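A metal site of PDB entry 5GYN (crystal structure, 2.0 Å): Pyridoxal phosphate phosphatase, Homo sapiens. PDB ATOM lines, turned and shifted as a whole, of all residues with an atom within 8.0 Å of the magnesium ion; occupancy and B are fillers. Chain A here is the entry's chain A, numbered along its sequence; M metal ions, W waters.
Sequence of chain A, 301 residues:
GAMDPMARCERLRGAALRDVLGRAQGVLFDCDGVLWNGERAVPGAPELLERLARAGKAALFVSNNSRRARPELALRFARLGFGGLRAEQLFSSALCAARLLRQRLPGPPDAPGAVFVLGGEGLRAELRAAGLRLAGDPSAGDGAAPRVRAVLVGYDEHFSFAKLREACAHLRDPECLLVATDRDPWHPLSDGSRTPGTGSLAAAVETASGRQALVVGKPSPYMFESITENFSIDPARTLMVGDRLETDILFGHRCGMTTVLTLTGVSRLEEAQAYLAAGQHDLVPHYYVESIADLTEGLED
The side-chain amino group of Lys 218 lies within salt-bridge range of the side-chain carboxylate of Asp 30, at 3.0 Å. The backbone NH of Asp 30 is in hydrogen-bond range of the backbone carbonyl oxygen of Val 241 (2.9 Å). The backbone NH of Asp 243 lies within hydrogen-bond range of the side-chain carboxylate of Asp 248. N of Val 266 sits at hydrogen-bond distance from OD2 of Asp 243 (2.7 Å). N of Ser 267 sits at hydrogen-bond distance from O of Asp 243 (2.9 Å). OD2 of Asp 248 sits at hydrogen-bond distance from N of Arg 244. The side-chain carboxylate of Asp 248 is in salt-bridge range of the side-chain amino group of Lys 218.
Residues that only touch the magnesium ion: Asp 248 (3.9 Å). Of the 27 residues printed, 4 come within 4 Å of the magnesium ion. Along chain A the residues within 4 Å of the magnesium ion span positions 30 to 248. The nearest printed residue that does not touch the magnesium ion is Gly 33 (4.4 Å).
OD2 of Asp 30 is bound to the magnesium ion (2.0 Å). OD1 of Asp 243 is bound to the magnesium ion (2.0 Å). The magnesium ion is bound by water W2 (2.0 Å). Water W1 binds the magnesium ion, 2.1 Å away. Water W3 binds the magnesium ion, at 2.1 Å. The magnesium ion is bound by O of Asp 32 (2.2 Å).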
ATOM      1  N   PHE A  29      12.860 -12.706   4.251  1.00  0.00           N
ATOM      2  CA  PHE A  29      13.201 -12.425   5.644  1.00  0.00           C
ATOM      3  C   PHE A  29      11.982 -12.393   6.573  1.00  0.00           C
ATOM      4  O   PHE A  29      11.028 -11.649   6.334  1.00  0.00           O
ATOM      5  CB  PHE A  29      13.888 -11.072   5.790  1.00  0.00           C
ATOM      6  CG  PHE A  29      15.265 -10.989   5.191  1.00  0.00           C
ATOM      7  CD1 PHE A  29      16.384 -11.367   5.920  1.00  0.00           C
ATOM      8  CD2 PHE A  29      15.441 -10.495   3.907  1.00  0.00           C
ATOM      9  CE1 PHE A  29      17.663 -11.275   5.362  1.00  0.00           C
ATOM     10  CE2 PHE A  29      16.712 -10.397   3.347  1.00  0.00           C
ATOM     11  CZ  PHE A  29      17.823 -10.787   4.075  1.00  0.00           C
ATOM     12  N   ASP A  30      12.028 -13.160   7.661  1.00  0.00           N
ATOM     13  CA  ASP A  30      11.174 -12.864   8.803  1.00  0.00           C
ATOM     14  C   ASP A  30      11.681 -11.537   9.378  1.00  0.00           C
ATOM     15  O   ASP A  30      12.810 -11.124   9.102  1.00  0.00           O
ATOM     16  CB  ASP A  30      11.235 -13.993   9.839  1.00  0.00           C
ATOM     17  CG  ASP A  30      10.576 -13.622  11.150  1.00  0.00           C
ATOM     18  OD1 ASP A  30       9.385 -13.240  11.137  1.00  0.00           O
ATOM     19  OD2 ASP A  30      11.266 -13.674  12.187  1.00  0.00           O
ATOM     20  N   CYS A  31      10.871 -10.843  10.177  1.00  0.00           N
ATOM     21  CA  CYS A  31      11.280  -9.527  10.672  1.00  0.00           C
ATOM     22  C   CYS A  31      11.779  -9.509  12.123  1.00  0.00           C
ATOM     23  O   CYS A  31      12.969  -9.325  12.375  1.00  0.00           O
ATOM     24  CB  CYS A  31      10.125  -8.537  10.506  1.00  0.00           C
ATOM     25  SG  CYS A  31       9.650  -8.242   8.770  1.00  0.00           S
ATOM     26  N   ASP A  32      10.868  -9.692  13.080  1.00  0.00           N
ATOM     27  CA  ASP A  32      11.225  -9.637  14.492  1.00  0.00           C
ATOM     28  C   ASP A  32      12.189 -10.775  14.852  1.00  0.00           C
ATOM     29  O   ASP A  32      11.940 -11.934  14.507  1.00  0.00           O
ATOM     30  CB  ASP A  32       9.978  -9.697  15.375  1.00  0.00           C
ATOM     31  CG  ASP A  32      10.165  -9.034  16.739  1.00  0.00           C
ATOM     32  OD1 ASP A  32      11.039  -8.156  16.875  1.00  0.00           O
ATOM     33  OD2 ASP A  32       9.432  -9.403  17.676  1.00  0.00           O
ATOM     34  N   GLY A  33      13.290 -10.438  15.517  1.00  0.00           N
ATOM     35  CA  GLY A  33      14.295 -11.429  15.853  1.00  0.00           C
ATOM     36  C   GLY A  33      15.276 -11.688  14.729  1.00  0.00           C
ATOM     37  O   GLY A  33      16.213 -12.478  14.875  1.00  0.00           O
ATOM     38  N   VAL A  34      15.075 -11.024  13.595  1.00  0.00           N
ATOM     39  CA  VAL A  34      15.927 -11.194  12.436  1.00  0.00           C
ATOM     40  C   VAL A  34      16.517  -9.864  11.975  1.00  0.00           C
ATOM     41  O   VAL A  34      17.730  -9.726  11.866  1.00  0.00           O
ATOM     42  CB  VAL A  34      15.159 -11.837  11.253  1.00  0.00           C
ATOM     43  CG1 VAL A  34      16.046 -11.914  10.009  1.00  0.00           C
ATOM     44  CG2 VAL A  34      14.633 -13.203  11.639  1.00  0.00           C
ATOM     45  N   LEU A  35      15.648  -8.899  11.713  1.00  0.00           N
ATOM     46  CA  LEU A  35      16.057  -7.567  11.289  1.00  0.00           C
ATOM     47  C   LEU A  35      16.277  -6.674  12.498  1.00  0.00           C
ATOM     48  O   LEU A  35      17.084  -5.738  12.464  1.00  0.00           O
ATOM     49  CB  LEU A  35      15.016  -6.929  10.376  1.00  0.00           C
ATOM     50  CG  LEU A  35      14.725  -7.650   9.075  1.00  0.00           C
ATOM     51  CD1 LEU A  35      13.668  -6.873   8.294  1.00  0.00           C
ATOM     52  CD2 LEU A  35      16.005  -7.795   8.286  1.00  0.00           C
ATOM     53  N   TRP A  36      15.524  -6.953  13.543  1.00  0.00           N
ATOM     54  CA  TRP A  36      15.558  -6.123  14.738  1.00  0.00           C
ATOM     55  C   TRP A  36      15.062  -6.895  15.947  1.00  0.00           C
ATOM     56  O   TRP A  36      14.529  -8.002  15.827  1.00  0.00           O
ATOM     57  CB  TRP A  36      14.696  -4.865  14.541  1.00  0.00           C
ATOM     58  CG  TRP A  36      13.287  -5.157  14.074  1.00  0.00           C
ATOM     59  CD1 TRP A  36      12.291  -5.779  14.792  1.00  0.00           C
ATOM     60  CD2 TRP A  36      12.709  -4.806  12.805  1.00  0.00           C
ATOM     61  NE1 TRP A  36      11.139  -5.852  14.027  1.00  0.00           N
ATOM     62  CE2 TRP A  36      11.375  -5.248  12.816  1.00  0.00           C
ATOM     63  CE3 TRP A  36      13.201  -4.158  11.671  1.00  0.00           C
ATOM     64  CZ2 TRP A  36      10.519  -5.077  11.731  1.00  0.00           C
ATOM     65  CZ3 TRP A  36      12.347  -3.981  10.593  1.00  0.00           C
ATOM     66  CH2 TRP A  36      11.027  -4.443  10.632  1.00  0.00           C
ATOM     67  N   ASN A  37      15.275  -6.304  17.114  1.00  0.00           N
ATOM     68  CA  ASN A  37      14.703  -6.800  18.363  1.00  0.00           C
ATOM     69  C   ASN A  37      14.142  -5.619  19.142  1.00  0.00           C
ATOM     70  O   ASN A  37      14.890  -4.874  19.771  1.00  0.00           O
ATOM     71  CB  ASN A  37      15.744  -7.523  19.199  1.00  0.00           C
ATOM     72  CG  ASN A  37      16.032  -8.909  18.682  1.00  0.00           C
ATOM     73  OD1 ASN A  37      15.129  -9.729  18.531  1.00  0.00           O
ATOM     74  ND2 ASN A  37      17.293  -9.179  18.396  1.00  0.00           N
ATOM     75  N   VAL A  62       8.318 -11.442   5.292  1.00  0.00           N
ATOM     76  CA  VAL A  62       7.165 -12.249   5.674  1.00  0.00           C
ATOM     77  C   VAL A  62       7.004 -12.242   7.196  1.00  0.00           C
ATOM     78  O   VAL A  62       7.859 -12.732   7.912  1.00  0.00           O
ATOM     79  CB  VAL A  62       7.300 -13.698   5.158  1.00  0.00           C
ATOM     80  CG1 VAL A  62       5.987 -14.405   5.239  1.00  0.00           C
ATOM     81  CG2 VAL A  62       7.788 -13.704   3.714  1.00  0.00           C
ATOM     82  N   SER A  63       5.904 -11.661   7.669  1.00  0.00           N
ATOM     83  CA  SER A  63       5.683 -11.464   9.108  1.00  0.00           C
ATOM     84  C   SER A  63       4.333 -12.037   9.558  1.00  0.00           C
ATOM     85  O   SER A  63       3.351 -11.957   8.828  1.00  0.00           O
ATOM     86  CB  SER A  63       5.757  -9.960   9.438  1.00  0.00           C
ATOM     87  OG  SER A  63       5.459  -9.721  10.809  1.00  0.00           O
ATOM     88  N   ASN A  64       4.283 -12.630  10.746  1.00  0.00           N
ATOM     89  CA  ASN A  64       3.010 -13.115  11.283  1.00  0.00           C
ATOM     90  C   ASN A  64       2.272 -12.041  12.071  1.00  0.00           C
ATOM     91  O   ASN A  64       1.317 -12.340  12.784  1.00  0.00           O
ATOM     92  CB  ASN A  64       3.223 -14.352  12.166  1.00  0.00           C
ATOM     93  CG  ASN A  64       3.243 -15.638  11.359  1.00  0.00           C
ATOM     94  OD1 ASN A  64       2.898 -15.643  10.178  1.00  0.00           O
ATOM     95  ND2 ASN A  64       3.627 -16.726  11.999  1.00  0.00           N
ATOM     96  N   ASP A 184       1.591 -18.577  16.567  1.00  0.00           N
ATOM     97  CA  ASP A 184       2.664 -18.231  17.489  1.00  0.00           C
ATOM     98  C   ASP A 184       2.122 -18.218  18.919  1.00  0.00           C
ATOM     99  O   ASP A 184       1.206 -17.466  19.238  1.00  0.00           O
ATOM    100  CB  ASP A 184       3.284 -16.884  17.128  1.00  0.00           C
ATOM    101  CG  ASP A 184       3.859 -16.861  15.723  1.00  0.00           C
ATOM    102  OD1 ASP A 184       4.178 -17.933  15.172  1.00  0.00           O
ATOM    103  OD2 ASP A 184       4.013 -15.748  15.172  1.00  0.00           O
ATOM    104  N   HIS A 187       5.369 -14.272  22.440  1.00  0.00           N
ATOM    105  CA  HIS A 187       6.432 -13.460  21.875  1.00  0.00           C
ATOM    106  C   HIS A 187       7.284 -12.832  22.970  1.00  0.00           C
ATOM    107  O   HIS A 187       6.758 -12.387  23.980  1.00  0.00           O
ATOM    108  CB  HIS A 187       5.843 -12.357  20.986  1.00  0.00           C
ATOM    109  CG  HIS A 187       4.995 -12.872  19.870  1.00  0.00           C
ATOM    110  ND1 HIS A 187       5.524 -13.437  18.730  1.00  0.00           N
ATOM    111  CD2 HIS A 187       3.645 -12.913  19.714  1.00  0.00           C
ATOM    112  CE1 HIS A 187       4.541 -13.803  17.920  1.00  0.00           C
ATOM    113  NE2 HIS A 187       3.390 -13.497  18.499  1.00  0.00           N
ATOM    114  N   PRO A 188       8.610 -12.792  22.768  1.00  0.00           N
ATOM    115  CA  PRO A 188       9.489 -12.161  23.752  1.00  0.00           C
ATOM    116  C   PRO A 188       9.351 -10.632  23.729  1.00  0.00           C
ATOM    117  O   PRO A 188       9.146 -10.048  22.656  1.00  0.00           O
ATOM    118  CB  PRO A 188      10.890 -12.591  23.308  1.00  0.00           C
ATOM    119  CG  PRO A 188      10.765 -12.817  21.828  1.00  0.00           C
ATOM    120  CD  PRO A 188       9.360 -13.345  21.621  1.00  0.00           C
ATOM    121  N   LYS A 218       2.820 -18.281   8.611  1.00  0.00           N
ATOM    122  CA  LYS A 218       3.849 -19.302   8.809  1.00  0.00           C
ATOM    123  C   LYS A 218       3.517 -20.101  10.053  1.00  0.00           C
ATOM    124  O   LYS A 218       3.094 -19.529  11.049  1.00  0.00           O
ATOM    125  CB  LYS A 218       5.235 -18.650   8.966  1.00  0.00           C
ATOM    126  CG  LYS A 218       5.723 -17.846   7.773  1.00  0.00           C
ATOM    127  CD  LYS A 218       6.868 -16.910   8.165  1.00  0.00           C
ATOM    128  CE  LYS A 218       6.426 -15.938   9.235  1.00  0.00           C
ATOM    129  NZ  LYS A 218       7.490 -14.976   9.618  1.00  0.00           N
ATOM    130  N   VAL A 241      15.095 -16.768   5.677  1.00  0.00           N
ATOM    131  CA  VAL A 241      15.862 -16.444   6.873  1.00  0.00           C
ATOM    132  C   VAL A 241      14.928 -16.124   8.036  1.00  0.00           C
ATOM    133  O   VAL A 241      14.100 -15.215   7.952  1.00  0.00           O
ATOM    134  CB  VAL A 241      16.802 -15.254   6.639  1.00  0.00           C
ATOM    135  CG1 VAL A 241      17.674 -15.018   7.864  1.00  0.00           C
ATOM    136  CG2 VAL A 241      17.682 -15.494   5.393  1.00  0.00           C
ATOM    137  N   GLY A 242      15.066 -16.871   9.129  1.00  0.00           N
ATOM    138  CA  GLY A 242      14.208 -16.661  10.281  1.00  0.00           C
ATOM    139  C   GLY A 242      14.874 -17.035  11.583  1.00  0.00           C
ATOM    140  O   GLY A 242      15.938 -17.657  11.582  1.00  0.00           O
ATOM    141  N   ASP A 243      14.255 -16.649  12.696  1.00  0.00           N
ATOM    142  CA  ASP A 243      14.813 -16.899  14.020  1.00  0.00           C
ATOM    143  C   ASP A 243      14.056 -17.977  14.775  1.00  0.00           C
ATOM    144  O   ASP A 243      14.501 -18.404  15.839  1.00  0.00           O
ATOM    145  CB  ASP A 243      14.804 -15.595  14.835  1.00  0.00           C
ATOM    146  CG  ASP A 243      13.401 -15.180  15.251  1.00  0.00           C
ATOM    147  OD1 ASP A 243      12.616 -14.815  14.355  1.00  0.00           O
ATOM    148  OD2 ASP A 243      13.071 -15.210  16.459  1.00  0.00           O
ATOM    149  N   ARG A 244      12.920 -18.417  14.246  1.00  0.00           N
ATOM    150  CA  ARG A 244      12.056 -19.342  14.969  1.00  0.00           C
ATOM    151  C   ARG A 244      11.846 -20.644  14.190  1.00  0.00           C
ATOM    152  O   ARG A 244      11.264 -20.643  13.105  1.00  0.00           O
ATOM    153  CB  ARG A 244      10.698 -18.682  15.268  1.00  0.00           C
ATOM    154  CG  ARG A 244       9.939 -19.315  16.417  1.00  0.00           C
ATOM    155  CD  ARG A 244       8.873 -18.372  16.953  1.00  0.00           C
ATOM    156  NE  ARG A 244       8.336 -18.843  18.236  1.00  0.00           N
ATOM    157  CZ  ARG A 244       7.610 -18.097  19.056  1.00  0.00           C
ATOM    158  NH1 ARG A 244       7.320 -16.829  18.738  1.00  0.00           N
ATOM    159  NH2 ARG A 244       7.172 -18.600  20.206  1.00  0.00           N
ATOM    160  N   THR A 247       8.319 -22.027  13.157  1.00  0.00           N
ATOM    161  CA  THR A 247       7.548 -21.092  12.350  1.00  0.00           C
ATOM    162  C   THR A 247       8.256 -20.810  11.023  1.00  0.00           C
ATOM    163  O   THR A 247       7.756 -21.164   9.969  1.00  0.00           O
ATOM    164  CB  THR A 247       7.304 -19.777  13.114  1.00  0.00           C
ATOM    165  OG1 THR A 247       6.449 -20.036  14.235  1.00  0.00           O
ATOM    166  CG2 THR A 247       6.644 -18.735  12.224  1.00  0.00           C
ATOM    167  N   ASP A 248       9.439 -20.216  11.110  1.00  0.00           N
ATOM    168  CA  ASP A 248      10.182 -19.771   9.931  1.00  0.00           C
ATOM    169  C   ASP A 248      10.840 -20.883   9.136  1.00  0.00           C
ATOM    170  O   ASP A 248      10.767 -20.913   7.906  1.00  0.00           O
ATOM    171  CB  ASP A 248      11.242 -18.756  10.364  1.00  0.00           C
ATOM    172  CG  ASP A 248      10.656 -17.609  11.142  1.00  0.00           C
ATOM    173  OD1 ASP A 248       9.600 -17.080  10.717  1.00  0.00           O
ATOM    174  OD2 ASP A 248      11.235 -17.225  12.182  1.00  0.00           O
ATOM    175  N   THR A 262      18.819 -17.602  12.022  1.00  0.00           N
ATOM    176  CA  THR A 262      19.649 -16.581  12.649  1.00  0.00           C
ATOM    177  C   THR A 262      19.460 -16.669  14.155  1.00  0.00           C
ATOM    178  O   THR A 262      18.370 -16.961  14.629  1.00  0.00           O
ATOM    179  CB  THR A 262      19.334 -15.162  12.128  1.00  0.00           C
ATOM    180  OG1 THR A 262      20.250 -14.231  12.722  1.00  0.00           O
ATOM    181  CG2 THR A 262      17.904 -14.760  12.481  1.00  0.00           C
ATOM    182  N   THR A 264      19.733 -14.392  16.520  1.00  0.00           N
ATOM    183  CA  THR A 264      19.378 -13.139  17.199  1.00  0.00           C
ATOM    184  C   THR A 264      17.939 -13.108  17.702  1.00  0.00           C
ATOM    185  O   THR A 264      17.448 -12.061  18.127  1.00  0.00           O
ATOM    186  CB  THR A 264      19.563 -11.916  16.267  1.00  0.00           C
ATOM    187  OG1 THR A 264      18.951 -12.186  15.006  1.00  0.00           O
ATOM    188  CG2 THR A 264      21.024 -11.631  16.029  1.00  0.00           C
ATOM    189  N   GLY A 265      17.244 -14.238  17.620  1.00  0.00           N
ATOM    190  CA  GLY A 265      15.830 -14.272  17.976  1.00  0.00           C
ATOM    191  C   GLY A 265      15.443 -15.337  18.978  1.00  0.00           C
ATOM    192  O   GLY A 265      16.124 -15.551  19.983  1.00  0.00           O
ATOM    193  N   VAL A 266      14.330 -16.011  18.699  1.00  0.00           N
ATOM    194  CA  VAL A 266      13.715 -16.930  19.663  1.00  0.00           C
ATOM    195  C   VAL A 266      14.431 -18.270  19.793  1.00  0.00           C
ATOM    196  O   VAL A 266      14.781 -18.681  20.906  1.00  0.00           O
ATOM    197  CB  VAL A 266      12.235 -17.183  19.299  1.00  0.00           C
ATOM    198  CG1 VAL A 266      11.662 -18.297  20.161  1.00  0.00           C
ATOM    199  CG2 VAL A 266      11.427 -15.902  19.457  1.00  0.00           C
ATOM    200  N   SER A 267      14.662 -18.958  18.679  1.00  0.00           N
ATOM    201  CA  SER A 267      15.222 -20.301  18.727  1.00  0.00           C
ATOM    202  C   SER A 267      16.733 -20.312  18.943  1.00  0.00           C
ATOM    203  O   SER A 267      17.443 -19.377  18.578  1.00  0.00           O
ATOM    204  CB  SER A 267      14.888 -21.069  17.444  1.00  0.00           C
ATOM    205  OG  SER A 267      13.492 -21.273  17.328  1.00  0.00           O
HETATM  206 MG    MG M   1      10.899 -13.824  14.113  1.00  0.00          MG
HETATM  207  O   HOH W   1       9.071 -12.882  14.013  1.00  0.00           O
HETATM  208  O   HOH W   2       9.859 -15.528  13.871  1.00  0.00           O
HETATM  209  O   HOH W   3      10.712 -14.080  16.155  1.00  0.00           O
